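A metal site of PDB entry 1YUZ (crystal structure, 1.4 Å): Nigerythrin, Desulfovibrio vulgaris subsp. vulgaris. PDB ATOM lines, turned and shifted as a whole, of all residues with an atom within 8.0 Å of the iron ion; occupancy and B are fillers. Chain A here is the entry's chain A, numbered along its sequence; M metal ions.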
ATOM      1  N   ILE A  75       3.541  23.175 -25.054  1.00  0.00           N
ATOM      2  CA  ILE A  75       3.173  24.461 -24.480  1.00  0.00           C
ATOM      3  C   ILE A  75       4.463  25.207 -24.148  1.00  0.00           C
ATOM      4  O   ILE A  75       4.588  26.401 -24.416  1.00  0.00           O
ATOM      5  CB  ILE A  75       2.323  24.274 -23.192  1.00  0.00           C
ATOM      6  CG1 ILE A  75       0.918  23.821 -23.573  1.00  0.00           C
ATOM      7  CG2 ILE A  75       2.265  25.582 -22.397  1.00  0.00           C
ATOM      8  CD1 ILE A  75       0.022  23.482 -22.396  1.00  0.00           C
ATOM      9  N   ARG A 144       8.336  29.109 -15.416  1.00  0.00           N
ATOM     10  CA  ARG A 144       7.092  28.375 -15.606  1.00  0.00           C
ATOM     11  C   ARG A 144       7.389  26.955 -16.091  1.00  0.00           C
ATOM     12  O   ARG A 144       6.818  25.986 -15.597  1.00  0.00           O
ATOM     13  CB  ARG A 144       6.207  29.125 -16.606  1.00  0.00           C
ATOM     14  CG  ARG A 144       4.819  28.549 -16.784  1.00  0.00           C
ATOM     15  CD  ARG A 144       3.813  29.641 -17.103  1.00  0.00           C
ATOM     16  NE  ARG A 144       3.578  30.500 -15.940  1.00  0.00           N
ATOM     17  CZ  ARG A 144       2.671  31.462 -15.883  1.00  0.00           C
ATOM     18  NH1 ARG A 144       1.881  31.700 -16.934  1.00  0.00           N
ATOM     19  NH2 ARG A 144       2.518  32.177 -14.774  1.00  0.00           N
ATOM     20  N   ALA A 148       6.945  23.052 -14.054  1.00  0.00           N
ATOM     21  CA  ALA A 148       6.165  21.958 -14.594  1.00  0.00           C
ATOM     22  C   ALA A 148       6.980  20.676 -14.700  1.00  0.00           C
ATOM     23  O   ALA A 148       6.463  19.587 -14.473  1.00  0.00           O
ATOM     24  CB  ALA A 148       5.618  22.323 -15.964  1.00  0.00           C
ATOM     25  N   LEU A 173      -4.386  18.859 -18.127  1.00  0.00           N
ATOM     26  CA  LEU A 173      -3.282  19.730 -18.498  1.00  0.00           C
ATOM     27  C   LEU A 173      -3.723  21.185 -18.499  1.00  0.00           C
ATOM     28  O   LEU A 173      -4.765  21.526 -19.056  1.00  0.00           O
ATOM     29  CB  LEU A 173      -2.762  19.349 -19.884  1.00  0.00           C
ATOM     30  CG  LEU A 173      -1.669  20.256 -20.461  1.00  0.00           C
ATOM     31  CD1 LEU A 173      -0.407  20.163 -19.603  1.00  0.00           C
ATOM     32  CD2 LEU A 173      -1.370  19.826 -21.891  1.00  0.00           C
ATOM     33  N   CYS A 174      -2.917  22.044 -17.884  1.00  0.00           N
ATOM     34  CA  CYS A 174      -3.204  23.459 -17.826  1.00  0.00           C
ATOM     35  C   CYS A 174      -3.174  24.059 -19.228  1.00  0.00           C
ATOM     36  O   CYS A 174      -2.431  23.592 -20.086  1.00  0.00           O
ATOM     37  CB  CYS A 174      -2.182  24.157 -16.929  1.00  0.00           C
ATOM     38  SG  CYS A 174      -2.375  25.937 -16.791  1.00  0.00           S
ATOM     39  N   PRO A 175      -3.982  25.084 -19.484  1.00  0.00           N
ATOM     40  CA  PRO A 175      -4.005  25.697 -20.814  1.00  0.00           C
ATOM     41  C   PRO A 175      -2.775  26.536 -21.166  1.00  0.00           C
ATOM     42  O   PRO A 175      -2.411  26.632 -22.332  1.00  0.00           O
ATOM     43  CB  PRO A 175      -5.276  26.554 -20.773  1.00  0.00           C
ATOM     44  CG  PRO A 175      -5.343  26.964 -19.342  1.00  0.00           C
ATOM     45  CD  PRO A 175      -5.028  25.667 -18.625  1.00  0.00           C
ATOM     46  N   ILE A 176      -2.118  27.116 -20.166  1.00  0.00           N
ATOM     47  CA  ILE A 176      -0.965  27.967 -20.426  1.00  0.00           C
ATOM     48  C   ILE A 176       0.376  27.548 -19.846  1.00  0.00           C
ATOM     49  O   ILE A 176       1.395  28.212 -20.082  1.00  0.00           O
ATOM     50  CB  ILE A 176      -1.261  29.430 -20.028  1.00  0.00           C
ATOM     51  CG1 ILE A 176      -1.485  29.525 -18.522  1.00  0.00           C
ATOM     52  CG2 ILE A 176      -2.489  29.927 -20.779  1.00  0.00           C
ATOM     53  CD1 ILE A 176      -1.638  30.947 -18.019  1.00  0.00           C
ATOM     54  N   CYS A 177       0.404  26.477 -19.064  1.00  0.00           N
ATOM     55  CA  CYS A 177       1.669  25.994 -18.526  1.00  0.00           C
ATOM     56  C   CYS A 177       1.651  24.474 -18.572  1.00  0.00           C
ATOM     57  O   CYS A 177       0.628  23.873 -18.938  1.00  0.00           O
ATOM     58  CB  CYS A 177       1.930  26.527 -17.111  1.00  0.00           C
ATOM     59  SG  CYS A 177       1.219  25.624 -15.730  1.00  0.00           S
ATOM     60  N   GLY A 178       2.758  23.851 -18.217  1.00  0.00           N
ATOM     61  CA  GLY A 178       2.842  22.407 -18.289  1.00  0.00           C
ATOM     62  C   GLY A 178       2.292  21.614 -17.132  1.00  0.00           C
ATOM     63  O   GLY A 178       2.447  20.390 -17.090  1.00  0.00           O
ATOM     64  N   TYR A 179       1.622  22.270 -16.193  1.00  0.00           N
ATOM     65  CA  TYR A 179       1.079  21.553 -15.048  1.00  0.00           C
ATOM     66  C   TYR A 179       0.089  20.458 -15.442  1.00  0.00           C
ATOM     67  O   TYR A 179      -0.802  20.680 -16.250  1.00  0.00           O
ATOM     68  CB  TYR A 179       0.398  22.507 -14.081  1.00  0.00           C
ATOM     69  CG  TYR A 179      -0.156  21.797 -12.869  1.00  0.00           C
ATOM     70  CD1 TYR A 179       0.690  21.250 -11.913  1.00  0.00           C
ATOM     71  CD2 TYR A 179      -1.536  21.655 -12.699  1.00  0.00           C
ATOM     72  CE1 TYR A 179       0.184  20.553 -10.817  1.00  0.00           C
ATOM     73  CE2 TYR A 179      -2.049  20.974 -11.600  1.00  0.00           C
ATOM     74  CZ  TYR A 179      -1.183  20.421 -10.670  1.00  0.00           C
ATOM     75  OH  TYR A 179      -1.696  19.761  -9.579  1.00  0.00           O
ATOM     76  N   ILE A 180       0.266  19.273 -14.847  1.00  0.00           N
ATOM     77  CA  ILE A 180      -0.626  18.153 -15.092  1.00  0.00           C
ATOM     78  C   ILE A 180      -1.124  17.623 -13.758  1.00  0.00           C
ATOM     79  O   ILE A 180      -0.347  17.399 -12.834  1.00  0.00           O
ATOM     80  CB  ILE A 180       0.103  16.995 -15.830  1.00  0.00           C
ATOM     81  CG1 ILE A 180       0.483  17.443 -17.240  1.00  0.00           C
ATOM     82  CG2 ILE A 180      -0.799  15.747 -15.882  1.00  0.00           C
ATOM     83  CD1 ILE A 180       1.405  16.480 -17.954  1.00  0.00           C
ATOM     84  N   LYS A 188      -7.442  24.689  -9.027  1.00  0.00           N
ATOM     85  CA  LYS A 188      -6.682  25.504  -9.963  1.00  0.00           C
ATOM     86  C   LYS A 188      -5.239  25.053 -10.080  1.00  0.00           C
ATOM     87  O   LYS A 188      -4.759  24.232  -9.294  1.00  0.00           O
ATOM     88  CB  LYS A 188      -6.722  26.969  -9.521  1.00  0.00           C
ATOM     89  CG  LYS A 188      -6.079  27.233  -8.168  1.00  0.00           C
ATOM     90  CD  LYS A 188      -6.109  28.724  -7.833  1.00  0.00           C
ATOM     91  CE  LYS A 188      -5.468  28.996  -6.487  1.00  0.00           C
ATOM     92  NZ  LYS A 188      -5.491  30.451  -6.147  1.00  0.00           N
ATOM     93  N   CYS A 189      -4.554  25.602 -11.072  1.00  0.00           N
ATOM     94  CA  CYS A 189      -3.149  25.284 -11.321  1.00  0.00           C
ATOM     95  C   CYS A 189      -2.258  25.907 -10.244  1.00  0.00           C
ATOM     96  O   CYS A 189      -2.340  27.100  -9.976  1.00  0.00           O
ATOM     97  CB  CYS A 189      -2.750  25.804 -12.694  1.00  0.00           C
ATOM     98  SG  CYS A 189      -1.047  25.456 -13.130  1.00  0.00           S
ATOM     99  N   PRO A 190      -1.401  25.097  -9.613  1.00  0.00           N
ATOM    100  CA  PRO A 190      -0.511  25.625  -8.574  1.00  0.00           C
ATOM    101  C   PRO A 190       0.654  26.444  -9.129  1.00  0.00           C
ATOM    102  O   PRO A 190       1.345  27.129  -8.380  1.00  0.00           O
ATOM    103  CB  PRO A 190      -0.034  24.368  -7.862  1.00  0.00           C
ATOM    104  CG  PRO A 190       0.055  23.383  -8.979  1.00  0.00           C
ATOM    105  CD  PRO A 190      -1.243  23.639  -9.735  1.00  0.00           C
ATOM    106  N   ILE A 191       0.848  26.381 -10.449  1.00  0.00           N
ATOM    107  CA  ILE A 191       1.929  27.128 -11.082  1.00  0.00           C
ATOM    108  C   ILE A 191       1.474  28.497 -11.601  1.00  0.00           C
ATOM    109  O   ILE A 191       2.161  29.487 -11.384  1.00  0.00           O
ATOM    110  CB  ILE A 191       2.538  26.320 -12.258  1.00  0.00           C
ATOM    111  CG1 ILE A 191       3.242  25.068 -11.709  1.00  0.00           C
ATOM    112  CG2 ILE A 191       3.525  27.191 -13.043  1.00  0.00           C
ATOM    113  CD1 ILE A 191       3.811  24.159 -12.787  1.00  0.00           C
ATOM    114  N   CYS A 192       0.325  28.537 -12.270  1.00  0.00           N
ATOM    115  CA  CYS A 192      -0.154  29.806 -12.824  1.00  0.00           C
ATOM    116  C   CYS A 192      -1.546  30.219 -12.324  1.00  0.00           C
ATOM    117  O   CYS A 192      -2.042  31.274 -12.712  1.00  0.00           O
ATOM    118  CB  CYS A 192      -0.170  29.737 -14.350  1.00  0.00           C
ATOM    119  SG  CYS A 192      -1.432  28.634 -15.006  1.00  0.00           S
ATOM    120  N   PHE A 193      -2.156  29.390 -11.491  1.00  0.00           N
ATOM    121  CA  PHE A 193      -3.473  29.676 -10.924  1.00  0.00           C
ATOM    122  C   PHE A 193      -4.680  29.562 -11.846  1.00  0.00           C
ATOM    123  O   PHE A 193      -5.798  29.906 -11.452  1.00  0.00           O
ATOM    124  CB  PHE A 193      -3.464  31.064 -10.255  1.00  0.00           C
ATOM    125  CG  PHE A 193      -2.809  31.077  -8.898  1.00  0.00           C
ATOM    126  CD1 PHE A 193      -1.985  30.040  -8.485  1.00  0.00           C
ATOM    127  CD2 PHE A 193      -3.021  32.154  -8.029  1.00  0.00           C
ATOM    128  CE1 PHE A 193      -1.364  30.071  -7.230  1.00  0.00           C
ATOM    129  CE2 PHE A 193      -2.402  32.192  -6.781  1.00  0.00           C
ATOM    130  CZ  PHE A 193      -1.572  31.147  -6.378  1.00  0.00           C
ATOM    131  N   ARG A 194      -4.482  29.090 -13.072  1.00  0.00           N
ATOM    132  CA  ARG A 194      -5.608  28.929 -13.993  1.00  0.00           C
ATOM    133  C   ARG A 194      -6.625  27.957 -13.374  1.00  0.00           C
ATOM    134  O   ARG A 194      -6.252  26.916 -12.849  1.00  0.00           O
ATOM    135  CB  ARG A 194      -5.133  28.386 -15.342  1.00  0.00           C
ATOM    136  CG  ARG A 194      -4.753  29.452 -16.348  1.00  0.00           C
ATOM    137  CD  ARG A 194      -5.985  30.182 -16.864  1.00  0.00           C
ATOM    138  NE  ARG A 194      -5.692  31.111 -17.955  1.00  0.00           N
ATOM    139  CZ  ARG A 194      -5.137  32.303 -17.785  1.00  0.00           C
ATOM    140  NH1 ARG A 194      -4.827  32.743 -16.565  1.00  0.00           N
ATOM    141  NH2 ARG A 194      -4.900  33.078 -18.840  1.00  0.00           N
ATOM    142  N   PRO A 195      -7.915  28.299 -13.438  1.00  0.00           N
ATOM    143  CA  PRO A 195      -8.968  27.434 -12.888  1.00  0.00           C
ATOM    144  C   PRO A 195      -9.082  26.093 -13.610  1.00  0.00           C
ATOM    145  O   PRO A 195      -8.811  25.993 -14.801  1.00  0.00           O
ATOM    146  CB  PRO A 195     -10.235  28.284 -13.028  1.00  0.00           C
ATOM    147  CG  PRO A 195      -9.708  29.693 -12.979  1.00  0.00           C
ATOM    148  CD  PRO A 195      -8.483  29.591 -13.856  1.00  0.00           C
ATOM    149  N   THR A 198     -10.487  25.452 -17.189  1.00  0.00           N
ATOM    150  CA  THR A 198      -9.762  25.806 -18.403  1.00  0.00           C
ATOM    151  C   THR A 198      -8.796  24.713 -18.854  1.00  0.00           C
ATOM    152  O   THR A 198      -8.162  24.828 -19.906  1.00  0.00           O
ATOM    153  CB  THR A 198      -8.965  27.115 -18.216  1.00  0.00           C
ATOM    154  OG1 THR A 198      -7.960  26.928 -17.204  1.00  0.00           O
ATOM    155  CG2 THR A 198      -9.895  28.243 -17.797  1.00  0.00           C
ATOM    156  N   PHE A 199      -8.673  23.666 -18.047  1.00  0.00           N
ATOM    157  CA  PHE A 199      -7.776  22.544 -18.348  1.00  0.00           C
ATOM    158  C   PHE A 199      -8.333  21.641 -19.441  1.00  0.00           C
ATOM    159  O   PHE A 199      -9.541  21.648 -19.722  1.00  0.00           O
ATOM    160  CB  PHE A 199      -7.539  21.700 -17.095  1.00  0.00           C
ATOM    161  CG  PHE A 199      -6.526  22.274 -16.146  1.00  0.00           C
ATOM    162  CD1 PHE A 199      -6.644  23.581 -15.666  1.00  0.00           C
ATOM    163  CD2 PHE A 199      -5.455  21.490 -15.710  1.00  0.00           C
ATOM    164  CE1 PHE A 199      -5.721  24.087 -14.760  1.00  0.00           C
ATOM    165  CE2 PHE A 199      -4.531  21.995 -14.804  1.00  0.00           C
ATOM    166  CZ  PHE A 199      -4.653  23.295 -14.330  1.00  0.00           C
HETATM  167 FE    FE M   1      -0.810  26.512 -15.219  1.00  0.00          FE
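The backbone NH of Arg 194 lies close to the side-chain sulfur of Cys 192, at 3.6 Å. N of Tyr 179 lies close to SG of Cys 177 (3.4 Å). The backbone NH of Cys 174 is in hydrogen-bond range of the backbone carbonyl oxygen of Tyr 179, at 3.0 Å. N of Ile 176 sits close to SG of Cys 174 (3.6 Å). The side-chain sulfur of Cys 189 lies close to the backbone NH of Ile 191. N of Cys 189 is in hydrogen-bond range of O of Arg 194, 2.8 Å away.
The iron ion is bound by the side-chain sulfur (SG) of Cys 192 (2.2 Å), the side-chain sulfur (SG) of Cys 177 (2.3 Å), the side-chain sulfur (SG) of Cys 174 (2.3 Å) and the side-chain sulfur (SG) of Cys 189 (2.4 Å). The iron ion has four donor atoms within binding distance.
Four residues have an atom within 4 Å of the iron ion: Cys 174, Cys 177, Cys 189 and Cys 192. The nearest printed residue that does not touch the iron ion is Tyr 179 (4.3 Å).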
